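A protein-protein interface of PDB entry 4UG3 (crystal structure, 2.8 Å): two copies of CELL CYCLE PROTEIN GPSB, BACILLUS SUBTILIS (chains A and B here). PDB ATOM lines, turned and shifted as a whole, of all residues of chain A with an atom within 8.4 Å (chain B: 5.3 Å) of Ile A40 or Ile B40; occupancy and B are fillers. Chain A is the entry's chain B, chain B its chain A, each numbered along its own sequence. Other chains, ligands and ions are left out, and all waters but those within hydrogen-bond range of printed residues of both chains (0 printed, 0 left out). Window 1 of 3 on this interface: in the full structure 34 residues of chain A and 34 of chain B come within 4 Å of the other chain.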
ATOM      1  N   VAL A   9       4.313   8.449 -12.390  1.00  0.00           N
ATOM      2  CA  VAL A   9       4.882   9.071 -13.581  1.00  0.00           C
ATOM      3  C   VAL A   9       6.289   9.638 -13.289  1.00  0.00           C
ATOM      4  O   VAL A   9       6.509  10.258 -12.263  1.00  0.00           O
ATOM      5  CB  VAL A   9       3.928  10.162 -14.129  1.00  0.00           C
ATOM      6  CG1 VAL A   9       4.544  10.902 -15.312  1.00  0.00           C
ATOM      7  CG2 VAL A   9       2.601   9.532 -14.529  1.00  0.00           C
ATOM      8  N   LYS A  10       7.211   9.417 -14.226  1.00  0.00           N
ATOM      9  CA  LYS A  10       8.626   9.767 -14.105  1.00  0.00           C
ATOM     10  C   LYS A  10       9.031  11.076 -14.792  1.00  0.00           C
ATOM     11  O   LYS A  10      10.132  11.554 -14.555  1.00  0.00           O
ATOM     12  CB  LYS A  10       9.486   8.646 -14.705  1.00  0.00           C
ATOM     13  CG  LYS A  10       9.409   7.295 -13.998  1.00  0.00           C
ATOM     14  CD  LYS A  10       9.956   6.183 -14.894  1.00  0.00           C
ATOM     15  CE  LYS A  10       9.996   4.819 -14.205  1.00  0.00           C
ATOM     16  NZ  LYS A  10       8.659   4.217 -13.922  1.00  0.00           N
ATOM     17  N   LEU A  11       8.191  11.636 -15.669  1.00  0.00           N
ATOM     18  CA  LEU A  11       8.499  12.903 -16.337  1.00  0.00           C
ATOM     19  C   LEU A  11       7.271  13.794 -16.487  1.00  0.00           C
ATOM     20  O   LEU A  11       6.164  13.307 -16.495  1.00  0.00           O
ATOM     21  CB  LEU A  11       9.098  12.640 -17.720  1.00  0.00           C
ATOM     22  CG  LEU A  11      10.495  12.048 -17.810  1.00  0.00           C
ATOM     23  CD1 LEU A  11      10.851  11.630 -19.230  1.00  0.00           C
ATOM     24  CD2 LEU A  11      11.511  13.043 -17.282  1.00  0.00           C
ATOM     25  N   SER A  12       7.489  15.100 -16.593  1.00  0.00           N
ATOM     26  CA  SER A  12       6.492  16.039 -17.062  1.00  0.00           C
ATOM     27  C   SER A  12       6.915  16.605 -18.417  1.00  0.00           C
ATOM     28  O   SER A  12       8.078  16.510 -18.822  1.00  0.00           O
ATOM     29  CB  SER A  12       6.334  17.186 -16.056  1.00  0.00           C
ATOM     30  OG  SER A  12       7.436  18.092 -16.073  1.00  0.00           O
ATOM     31  N   ALA A  13       5.961  17.219 -19.101  1.00  0.00           N
ATOM     32  CA  ALA A  13       6.234  18.005 -20.300  1.00  0.00           C
ATOM     33  C   ALA A  13       7.373  18.980 -20.051  1.00  0.00           C
ATOM     34  O   ALA A  13       8.347  19.043 -20.820  1.00  0.00           O
ATOM     35  CB  ALA A  13       4.988  18.777 -20.716  1.00  0.00           C
ATOM     36  N   ILE A  16      10.779  17.338 -20.019  1.00  0.00           N
ATOM     37  CA  ILE A  16      11.221  16.986 -21.399  1.00  0.00           C
ATOM     38  C   ILE A  16      11.630  18.234 -22.197  1.00  0.00           C
ATOM     39  O   ILE A  16      12.685  18.243 -22.813  1.00  0.00           O
ATOM     40  CB  ILE A  16      10.157  16.224 -22.211  1.00  0.00           C
ATOM     41  CG1 ILE A  16       9.791  14.895 -21.537  1.00  0.00           C
ATOM     42  CG2 ILE A  16      10.669  15.947 -23.614  1.00  0.00           C
ATOM     43  CD1 ILE A  16       8.548  14.229 -22.088  1.00  0.00           C
ATOM     44  N   PHE A  21      20.886  17.460 -23.085  1.00  0.00           N
ATOM     45  CA  PHE A  21      21.742  16.287 -23.156  1.00  0.00           C
ATOM     46  C   PHE A  21      23.216  16.648 -23.229  1.00  0.00           C
ATOM     47  O   PHE A  21      23.584  17.743 -23.659  1.00  0.00           O
ATOM     48  CB  PHE A  21      21.371  15.413 -24.347  1.00  0.00           C
ATOM     49  CG  PHE A  21      20.019  14.783 -24.228  1.00  0.00           C
ATOM     50  CD1 PHE A  21      19.814  13.691 -23.382  1.00  0.00           C
ATOM     51  CD2 PHE A  21      18.946  15.280 -24.941  1.00  0.00           C
ATOM     52  CE1 PHE A  21      18.553  13.128 -23.253  1.00  0.00           C
ATOM     53  CE2 PHE A  21      17.697  14.708 -24.820  1.00  0.00           C
ATOM     54  CZ  PHE A  21      17.492  13.635 -23.983  1.00  0.00           C
ATOM     55  N   VAL A  33      16.325  14.659 -32.851  1.00  0.00           N
ATOM     56  CA  VAL A  33      15.913  14.348 -31.482  1.00  0.00           C
ATOM     57  C   VAL A  33      14.887  15.356 -30.931  1.00  0.00           C
ATOM     58  O   VAL A  33      13.892  14.950 -30.325  1.00  0.00           O
ATOM     59  CB  VAL A  33      17.121  14.276 -30.521  1.00  0.00           C
ATOM     60  CG1 VAL A  33      16.672  14.082 -29.076  1.00  0.00           C
ATOM     61  CG2 VAL A  33      18.049  13.137 -30.929  1.00  0.00           C
ATOM     62  N   ASP A  34      15.125  16.647 -31.166  1.00  0.00           N
ATOM     63  CA  ASP A  34      14.208  17.674 -30.712  1.00  0.00           C
ATOM     64  C   ASP A  34      12.810  17.480 -31.338  1.00  0.00           C
ATOM     65  O   ASP A  34      11.793  17.507 -30.632  1.00  0.00           O
ATOM     66  CB  ASP A  34      14.758  19.076 -30.988  1.00  0.00           C
ATOM     67  CG  ASP A  34      16.105  19.362 -30.281  1.00  0.00           C
ATOM     68  OD1 ASP A  34      16.479  18.659 -29.313  1.00  0.00           O
ATOM     69  OD2 ASP A  34      16.802  20.329 -30.689  1.00  0.00           O
ATOM     70  N   LYS A  35      12.766  17.242 -32.648  1.00  0.00           N
ATOM     71  CA  LYS A  35      11.491  17.017 -33.362  1.00  0.00           C
ATOM     72  C   LYS A  35      10.706  15.822 -32.819  1.00  0.00           C
ATOM     73  O   LYS A  35       9.463  15.869 -32.713  1.00  0.00           O
ATOM     74  CB  LYS A  35      11.721  16.833 -34.863  1.00  0.00           C
ATOM     75  CG  LYS A  35      12.010  18.112 -35.623  1.00  0.00           C
ATOM     76  CD  LYS A  35      12.083  17.853 -37.112  1.00  0.00           C
ATOM     77  CE  LYS A  35      12.836  18.948 -37.851  1.00  0.00           C
ATOM     78  NZ  LYS A  35      12.954  18.724 -39.327  1.00  0.00           N
ATOM     79  N   PHE A  36      11.430  14.764 -32.476  1.00  0.00           N
ATOM     80  CA  PHE A  36      10.821  13.587 -31.920  1.00  0.00           C
ATOM     81  C   PHE A  36      10.374  13.846 -30.483  1.00  0.00           C
ATOM     82  O   PHE A  36       9.239  13.530 -30.113  1.00  0.00           O
ATOM     83  CB  PHE A  36      11.814  12.455 -31.977  1.00  0.00           C
ATOM     84  CG  PHE A  36      11.198  11.094 -31.888  1.00  0.00           C
ATOM     85  CD1 PHE A  36      10.544  10.563 -32.974  1.00  0.00           C
ATOM     86  CD2 PHE A  36      11.324  10.322 -30.727  1.00  0.00           C
ATOM     87  CE1 PHE A  36      10.006   9.294 -32.917  1.00  0.00           C
ATOM     88  CE2 PHE A  36      10.792   9.049 -30.663  1.00  0.00           C
ATOM     89  CZ  PHE A  36      10.129   8.534 -31.761  1.00  0.00           C
ATOM     90  N   LEU A  37      11.253  14.442 -29.678  1.00  0.00           N
ATOM     91  CA  LEU A  37      10.879  14.886 -28.320  1.00  0.00           C
ATOM     92  C   LEU A  37       9.640  15.792 -28.319  1.00  0.00           C
ATOM     93  O   LEU A  37       8.737  15.662 -27.468  1.00  0.00           O
ATOM     94  CB  LEU A  37      12.057  15.575 -27.608  1.00  0.00           C
ATOM     95  CG  LEU A  37      13.159  14.617 -27.102  1.00  0.00           C
ATOM     96  CD1 LEU A  37      14.253  15.315 -26.318  1.00  0.00           C
ATOM     97  CD2 LEU A  37      12.597  13.478 -26.270  1.00  0.00           C
ATOM     98  N   ASP A  38       9.597  16.674 -29.308  1.00  0.00           N
ATOM     99  CA  ASP A  38       8.469  17.548 -29.512  1.00  0.00           C
ATOM    100  C   ASP A  38       7.174  16.825 -29.796  1.00  0.00           C
ATOM    101  O   ASP A  38       6.123  17.277 -29.320  1.00  0.00           O
ATOM    102  CB  ASP A  38       8.739  18.490 -30.670  1.00  0.00           C
ATOM    103  CG  ASP A  38       7.636  19.456 -30.866  1.00  0.00           C
ATOM    104  OD1 ASP A  38       7.189  20.017 -29.834  1.00  0.00           O
ATOM    105  OD2 ASP A  38       7.193  19.619 -32.026  1.00  0.00           O
ATOM    106  N   MET A  39       7.241  15.750 -30.600  1.00  0.00           N
ATOM    107  CA  MET A  39       6.088  14.858 -30.790  1.00  0.00           C
ATOM    108  C   MET A  39       5.645  14.269 -29.464  1.00  0.00           C
ATOM    109  O   MET A  39       4.519  14.421 -29.057  1.00  0.00           O
ATOM    110  CB  MET A  39       6.398  13.723 -31.754  1.00  0.00           C
ATOM    111  CG  MET A  39       5.900  13.974 -33.165  1.00  0.00           C
ATOM    112  SD  MET A  39       6.389  12.654 -34.282  1.00  0.00           S
ATOM    113  CE  MET A  39       7.980  13.295 -34.852  1.00  0.00           C
ATOM    114  N   ILE A  40       6.569  13.620 -28.784  1.00  0.00           N
ATOM    115  CA  ILE A  40       6.306  13.036 -27.476  1.00  0.00           C
ATOM    116  C   ILE A  40       5.656  14.007 -26.473  1.00  0.00           C
ATOM    117  O   ILE A  40       4.765  13.602 -25.724  1.00  0.00           O
ATOM    118  CB  ILE A  40       7.618  12.469 -26.876  1.00  0.00           C
ATOM    119  CG1 ILE A  40       8.035  11.220 -27.644  1.00  0.00           C
ATOM    120  CG2 ILE A  40       7.479  12.148 -25.385  1.00  0.00           C
ATOM    121  CD1 ILE A  40       9.531  10.975 -27.602  1.00  0.00           C
ATOM    122  N   ILE A  41       6.129  15.251 -26.427  1.00  0.00           N
ATOM    123  CA  ILE A  41       5.560  16.243 -25.528  1.00  0.00           C
ATOM    124  C   ILE A  41       4.065  16.406 -25.800  1.00  0.00           C
ATOM    125  O   ILE A  41       3.265  16.325 -24.874  1.00  0.00           O
ATOM    126  CB  ILE A  41       6.299  17.593 -25.652  1.00  0.00           C
ATOM    127  CG1 ILE A  41       7.608  17.547 -24.867  1.00  0.00           C
ATOM    128  CG2 ILE A  41       5.440  18.778 -25.214  1.00  0.00           C
ATOM    129  CD1 ILE A  41       8.650  18.477 -25.448  1.00  0.00           C
ATOM    130  N   LYS A  42       3.691  16.592 -27.062  1.00  0.00           N
ATOM    131  CA  LYS A  42       2.284  16.751 -27.440  1.00  0.00           C
ATOM    132  C   LYS A  42       1.421  15.546 -27.070  1.00  0.00           C
ATOM    133  O   LYS A  42       0.214  15.687 -26.790  1.00  0.00           O
ATOM    134  CB  LYS A  42       2.145  16.996 -28.944  1.00  0.00           C
ATOM    135  CG  LYS A  42       2.684  18.336 -29.430  1.00  0.00           C
ATOM    136  CD  LYS A  42       2.574  18.436 -30.954  1.00  0.00           C
ATOM    137  CE  LYS A  42       3.597  19.387 -31.554  1.00  0.00           C
ATOM    138  NZ  LYS A  42       3.858  19.100 -32.990  1.00  0.00           N
ATOM    139  N   ASP A  43       2.023  14.363 -27.114  1.00  0.00           N
ATOM    140  CA  ASP A  43       1.360  13.158 -26.651  1.00  0.00           C
ATOM    141  C   ASP A  43       1.134  13.198 -25.131  1.00  0.00           C
ATOM    142  O   ASP A  43       0.077  12.774 -24.660  1.00  0.00           O
ATOM    143  CB  ASP A  43       2.138  11.893 -27.060  1.00  0.00           C
ATOM    144  CG  ASP A  43       1.967  11.527 -28.542  1.00  0.00           C
ATOM    145  OD1 ASP A  43       1.236  12.212 -29.287  1.00  0.00           O
ATOM    146  OD2 ASP A  43       2.599  10.543 -28.959  1.00  0.00           O
ATOM    147  N   TYR A  44       2.117  13.700 -24.372  1.00  0.00           N
ATOM    148  CA  TYR A  44       1.955  13.818 -22.933  1.00  0.00           C
ATOM    149  C   TYR A  44       0.746  14.669 -22.643  1.00  0.00           C
ATOM    150  O   TYR A  44      -0.012  14.383 -21.727  1.00  0.00           O
ATOM    151  CB  TYR A  44       3.185  14.430 -22.250  1.00  0.00           C
ATOM    152  CG  TYR A  44       4.234  13.436 -21.789  1.00  0.00           C
ATOM    153  CD1 TYR A  44       4.829  12.577 -22.692  1.00  0.00           C
ATOM    154  CD2 TYR A  44       4.648  13.386 -20.447  1.00  0.00           C
ATOM    155  CE1 TYR A  44       5.797  11.692 -22.297  1.00  0.00           C
ATOM    156  CE2 TYR A  44       5.625  12.489 -20.030  1.00  0.00           C
ATOM    157  CZ  TYR A  44       6.202  11.646 -20.975  1.00  0.00           C
ATOM    158  OH  TYR A  44       7.166  10.733 -20.631  1.00  0.00           O
ATOM    159  N   GLU A  45       0.564  15.704 -23.440  1.00  0.00           N
ATOM    160  CA  GLU A  45      -0.511  16.663 -23.232  1.00  0.00           C
ATOM    161  C   GLU A  45      -1.843  16.010 -23.489  1.00  0.00           C
ATOM    162  O   GLU A  45      -2.773  16.121 -22.695  1.00  0.00           O
ATOM    163  CB  GLU A  45      -0.271  17.903 -24.099  1.00  0.00           C
ATOM    164  CG  GLU A  45       1.061  18.568 -23.698  1.00  0.00           C
ATOM    165  CD  GLU A  45       1.321  19.939 -24.301  1.00  0.00           C
ATOM    166  OE1 GLU A  45       0.715  20.273 -25.358  1.00  0.00           O
ATOM    167  OE2 GLU A  45       2.159  20.663 -23.700  1.00  0.00           O
ATOM    168  N   THR A  46      -1.890  15.271 -24.585  1.00  0.00           N
ATOM    169  CA  THR A  46      -3.076  14.519 -24.998  1.00  0.00           C
ATOM    170  C   THR A  46      -3.518  13.511 -23.937  1.00  0.00           C
ATOM    171  O   THR A  46      -4.697  13.452 -23.600  1.00  0.00           O
ATOM    172  CB  THR A  46      -2.813  13.861 -26.369  1.00  0.00           C
ATOM    173  OG1 THR A  46      -2.945  14.871 -27.370  1.00  0.00           O
ATOM    174  CG2 THR A  46      -3.772  12.729 -26.680  1.00  0.00           C
ATOM    175  N   PHE A  47      -2.555  12.748 -23.423  1.00  0.00           N
ATOM    176  CA  PHE A  47      -2.781  11.798 -22.355  1.00  0.00           C
ATOM    177  C   PHE A  47      -3.423  12.425 -21.134  1.00  0.00           C
ATOM    178  O   PHE A  47      -4.325  11.827 -20.546  1.00  0.00           O
ATOM    179  CB  PHE A  47      -1.477  11.099 -21.932  1.00  0.00           C
ATOM    180  CG  PHE A  47      -1.002  10.022 -22.895  1.00  0.00           C
ATOM    181  CD1 PHE A  47      -1.846   8.979 -23.276  1.00  0.00           C
ATOM    182  CD2 PHE A  47       0.312  10.022 -23.371  1.00  0.00           C
ATOM    183  CE1 PHE A  47      -1.415   7.988 -24.163  1.00  0.00           C
ATOM    184  CE2 PHE A  47       0.756   9.030 -24.240  1.00  0.00           C
ATOM    185  CZ  PHE A  47      -0.109   8.015 -24.650  1.00  0.00           C
ATOM    186  N   LEU B  11       2.336   8.669 -31.508  1.00  0.00           N
ATOM    187  CA  LEU B  11       3.340   7.593 -31.430  1.00  0.00           C
ATOM    188  C   LEU B  11       2.923   6.473 -30.503  1.00  0.00           C
ATOM    189  O   LEU B  11       2.061   6.650 -29.655  1.00  0.00           O
ATOM    190  CB  LEU B  11       4.664   8.138 -30.909  1.00  0.00           C
ATOM    191  CG  LEU B  11       5.494   9.013 -31.839  1.00  0.00           C
ATOM    192  CD1 LEU B  11       6.618   9.688 -31.057  1.00  0.00           C
ATOM    193  CD2 LEU B  11       6.043   8.207 -33.012  1.00  0.00           C
ATOM    194  N   ILE B  16       8.721   4.401 -30.440  1.00  0.00           N
ATOM    195  CA  ILE B  16       9.748   5.141 -29.710  1.00  0.00           C
ATOM    196  C   ILE B  16      10.988   4.277 -29.567  1.00  0.00           C
ATOM    197  O   ILE B  16      12.095   4.716 -29.885  1.00  0.00           O
ATOM    198  CB  ILE B  16       9.252   5.600 -28.318  1.00  0.00           C
ATOM    199  CG1 ILE B  16       8.152   6.653 -28.467  1.00  0.00           C
ATOM    200  CG2 ILE B  16      10.381   6.209 -27.509  1.00  0.00           C
ATOM    201  CD1 ILE B  16       7.304   6.841 -27.221  1.00  0.00           C
ATOM    202  N   PHE B  36      16.780   8.292 -21.434  1.00  0.00           N
ATOM    203  CA  PHE B  36      15.661   9.194 -21.341  1.00  0.00           C
ATOM    204  C   PHE B  36      14.450   8.613 -22.107  1.00  0.00           C
ATOM    205  O   PHE B  36      13.322   8.634 -21.606  1.00  0.00           O
ATOM    206  CB  PHE B  36      16.094  10.557 -21.868  1.00  0.00           C
ATOM    207  CG  PHE B  36      15.258  11.696 -21.382  1.00  0.00           C
ATOM    208  CD1 PHE B  36      15.325  12.103 -20.067  1.00  0.00           C
ATOM    209  CD2 PHE B  36      14.432  12.398 -22.253  1.00  0.00           C
ATOM    210  CE1 PHE B  36      14.556  13.174 -19.607  1.00  0.00           C
ATOM    211  CE2 PHE B  36      13.665  13.470 -21.807  1.00  0.00           C
ATOM    212  CZ  PHE B  36      13.727  13.859 -20.478  1.00  0.00           C
ATOM    213  N   LEU B  37      14.679   8.044 -23.294  1.00  0.00           N
ATOM    214  CA  LEU B  37      13.589   7.402 -24.046  1.00  0.00           C
ATOM    215  C   LEU B  37      12.967   6.210 -23.320  1.00  0.00           C
ATOM    216  O   LEU B  37      11.800   5.938 -23.515  1.00  0.00           O
ATOM    217  CB  LEU B  37      14.046   6.975 -25.443  1.00  0.00           C
ATOM    218  CG  LEU B  37      14.309   8.036 -26.519  1.00  0.00           C
ATOM    219  CD1 LEU B  37      14.337   7.356 -27.877  1.00  0.00           C
ATOM    220  CD2 LEU B  37      13.300   9.184 -26.545  1.00  0.00           C
ATOM    221  N   ASP B  38      13.746   5.506 -22.499  1.00  0.00           N
ATOM    222  CA  ASP B  38      13.212   4.453 -21.632  1.00  0.00           C
ATOM    223  C   ASP B  38      12.272   4.988 -20.576  1.00  0.00           C
ATOM    224  O   ASP B  38      11.222   4.401 -20.339  1.00  0.00           O
ATOM    225  CB  ASP B  38      14.324   3.632 -20.945  1.00  0.00           C
ATOM    226  CG  ASP B  38      15.110   2.753 -21.919  1.00  0.00           C
ATOM    227  OD1 ASP B  38      14.526   2.144 -22.845  1.00  0.00           O
ATOM    228  OD2 ASP B  38      16.334   2.668 -21.730  1.00  0.00           O
ATOM    229  N   MET B  39      12.643   6.074 -19.918  1.00  0.00           N
ATOM    230  CA  MET B  39      11.708   6.714 -18.992  1.00  0.00           C
ATOM    231  C   MET B  39      10.378   7.027 -19.693  1.00  0.00           C
ATOM    232  O   MET B  39       9.307   6.799 -19.124  1.00  0.00           O
ATOM    233  CB  MET B  39      12.299   7.988 -18.384  1.00  0.00           C
ATOM    234  CG  MET B  39      13.365   7.726 -17.346  1.00  0.00           C
ATOM    235  SD  MET B  39      14.122   9.248 -16.750  1.00  0.00           S
ATOM    236  CE  MET B  39      12.996   9.704 -15.431  1.00  0.00           C
ATOM    237  N   ILE B  40      10.457   7.522 -20.928  1.00  0.00           N
ATOM    238  CA  ILE B  40       9.280   7.962 -21.664  1.00  0.00           C
ATOM    239  C   ILE B  40       8.338   6.788 -21.943  1.00  0.00           C
ATOM    240  O   ILE B  40       7.133   6.883 -21.716  1.00  0.00           O
ATOM    241  CB  ILE B  40       9.683   8.719 -22.971  1.00  0.00           C
ATOM    242  CG1 ILE B  40      10.240  10.101 -22.629  1.00  0.00           C
ATOM    243  CG2 ILE B  40       8.486   8.894 -23.911  1.00  0.00           C
ATOM    244  CD1 ILE B  40      11.019  10.768 -23.728  1.00  0.00           C
ATOM    245  N   ILE B  41       8.922   5.695 -22.426  1.00  0.00           N
ATOM    246  CA  ILE B  41       8.224   4.420 -22.667  1.00  0.00           C
ATOM    247  C   ILE B  41       7.480   3.947 -21.438  1.00  0.00           C
ATOM    248  O   ILE B  41       6.376   3.429 -21.561  1.00  0.00           O
ATOM    249  CB  ILE B  41       9.223   3.313 -23.122  1.00  0.00           C
ATOM    250  CG1 ILE B  41       9.705   3.594 -24.553  1.00  0.00           C
ATOM    251  CG2 ILE B  41       8.603   1.928 -23.072  1.00  0.00           C
ATOM    252  CD1 ILE B  41      11.101   3.097 -24.861  1.00  0.00           C
ATOM    253  N   LYS B  42       8.097   4.101 -20.267  1.00  0.00           N
ATOM    254  CA  LYS B  42       7.449   3.761 -19.015  1.00  0.00           C
ATOM    255  C   LYS B  42       6.239   4.643 -18.797  1.00  0.00           C
ATOM    256  O   LYS B  42       5.177   4.141 -18.449  1.00  0.00           O
ATOM    257  CB  LYS B  42       8.423   3.838 -17.837  1.00  0.00           C
ATOM    258  CG  LYS B  42       9.197   2.539 -17.679  1.00  0.00           C
ATOM    259  CD  LYS B  42      10.650   2.710 -17.260  1.00  0.00           C
ATOM    260  CE  LYS B  42      11.555   1.763 -18.054  1.00  0.00           C
ATOM    261  NZ  LYS B  42      12.853   1.496 -17.371  1.00  0.00           N
ATOM    262  N   ASP B  43       6.391   5.943 -19.043  1.00  0.00           N
ATOM    263  CA  ASP B  43       5.289   6.878 -18.913  1.00  0.00           C
ATOM    264  C   ASP B  43       4.113   6.564 -19.855  1.00  0.00           C
ATOM    265  O   ASP B  43       2.961   6.598 -19.409  1.00  0.00           O
ATOM    266  CB  ASP B  43       5.792   8.311 -19.071  1.00  0.00           C
ATOM    267  CG  ASP B  43       6.596   8.799 -17.851  1.00  0.00           C
ATOM    268  OD1 ASP B  43       6.930   7.991 -16.960  1.00  0.00           O
ATOM    269  OD2 ASP B  43       6.912  10.000 -17.780  1.00  0.00           O
ATOM    270  N   TYR B  44       4.402   6.220 -21.117  1.00  0.00           N
ATOM    271  CA  TYR B  44       3.369   5.778 -22.094  1.00  0.00           C
ATOM    272  C   TYR B  44       2.572   4.569 -21.626  1.00  0.00           C
ATOM    273  O   TYR B  44       1.362   4.507 -21.810  1.00  0.00           O
ATOM    274  CB  TYR B  44       3.969   5.431 -23.469  1.00  0.00           C
ATOM    275  CG  TYR B  44       4.093   6.604 -24.421  1.00  0.00           C
ATOM    276  CD1 TYR B  44       4.785   7.775 -24.052  1.00  0.00           C
ATOM    277  CD2 TYR B  44       3.551   6.549 -25.703  1.00  0.00           C
ATOM    278  CE1 TYR B  44       4.928   8.839 -24.932  1.00  0.00           C
ATOM    279  CE2 TYR B  44       3.684   7.622 -26.579  1.00  0.00           C
ATOM    280  CZ  TYR B  44       4.370   8.754 -26.178  1.00  0.00           C
ATOM    281  OH  TYR B  44       4.487   9.787 -27.036  1.00  0.00           O
ATOM    282  N   GLU B  45       3.275   3.601 -21.057  1.00  0.00           N
ATOM    283  CA  GLU B  45       2.625   2.424 -20.505  1.00  0.00           C
ATOM    284  C   GLU B  45       1.756   2.827 -19.308  1.00  0.00           C
ATOM    285  O   GLU B  45       0.606   2.391 -19.207  1.00  0.00           O
ATOM    286  CB  GLU B  45       3.679   1.396 -20.111  1.00  0.00           C
ATOM    287  CG  GLU B  45       3.157   0.078 -19.537  1.00  0.00           C
ATOM    288  CD  GLU B  45       4.274  -0.836 -19.038  1.00  0.00           C
ATOM    289  OE1 GLU B  45       5.457  -0.524 -19.292  1.00  0.00           O
ATOM    290  OE2 GLU B  45       3.978  -1.863 -18.390  1.00  0.00           O
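The backbone NH of Leu B11 sits at hydrogen-bond distance from the side-chain carboxylate of Asp A43 (3.2 Å). The backbone NH (N) of Lys A10 lies within hydrogen-bond range of the side-chain carboxylate (OD1) of Asp B43 (3.1 Å). The side-chain carboxylate of Asp B43 is in hydrogen-bond range of the backbone NH of Leu A11 (3.0 Å). The side-chain carboxylate (OD2) of Asp B43 is in hydrogen-bond range of the side-chain hydroxyl (OH) of Tyr A44 (3.0 Å). The side-chain carboxylate (OD2) of Asp A43 sits at hydrogen-bond distance from the side-chain hydroxyl (OH) of Tyr B44 (2.8 Å).
Among the printed residues, merely in contact across the chains: Val A9 with Asp B43 (3.5 Å), Lys A10 with Met B39 (3.5 Å), Lys A10 with Lys B42 (3.8 Å), Leu A11 with Phe B36 (3.8 Å), Leu A11 with Ile B40 (3.8 Å), Phe A21 with Phe B36 (3.7 Å), Phe A36 with Leu B11 (3.8 Å), Phe A36 with Ile B16 (3.98 Å), Ile A40 with Ile B40 (3.7 Å), Ile A40 with Tyr B44 (3.7 Å), Tyr A44 with Ile B40 (3.6 Å) and Tyr A44 with Tyr B44 (3.98 Å).
Printed residues of chain B within 4 Å of Phe A21: Phe B36. Printed residues of chain B within 4 Å of Phe A36: Leu B11 (3.8 Å) and Ile B16 (3.98 Å). Ile B40 touches just these residues of chain A: Leu A11 (3.8 Å), Ile A40 (3.7 Å) and Tyr A44 (3.6 Å). Of the printed residues of chain A, Lys B42 touches Lys A10 (3.8 Å). The nearest printed residue of chain B that does not touch Ile A40 is Leu B11 (4.0004 Å). The nearest residue of chain A that does not touch Ile B40 is Leu A37 (4.04 Å). The nearest printed residue of chain B that does not touch Val A9 is Lys B42 (6.9 Å).
Hydrophobic or aromatic side chains of chain B within 4 Å of the printed part of chain A: Leu B11, Phe B36, Met B39, Ile B40 and Tyr B44. Of the 22 printed residues of chain A, 8 touch a printed residue of chain B. Among the printed residues, 17 pairs touch across the chains. Among the printed residues, no Asp or Glu carboxylate lies within 4 Å of a Lys or Arg side-chain nitrogen of the other chain.
Leu A11 touches Phe B36, and with the chains exchanged Phe A36 touches Leu B11. Phe A36 touches Ile B16, but with the chains exchanged Ile A16 does not touch Phe B36 (4.1 Å). Ile A40 touches Tyr B44, and with the chains exchanged Tyr A44 touches Ile B40. Asp A43 touches Tyr B44, and with the chains exchanged Tyr A44 touches Asp B43. Positions printed for both chains: 11, 16, 36, 37, 38, 39, 40, 41, 42, 43, 44 and 45. Of the 17 pairs that touch across the chains among the printed residues, 10 have their exchanged pair printed and touching as well.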
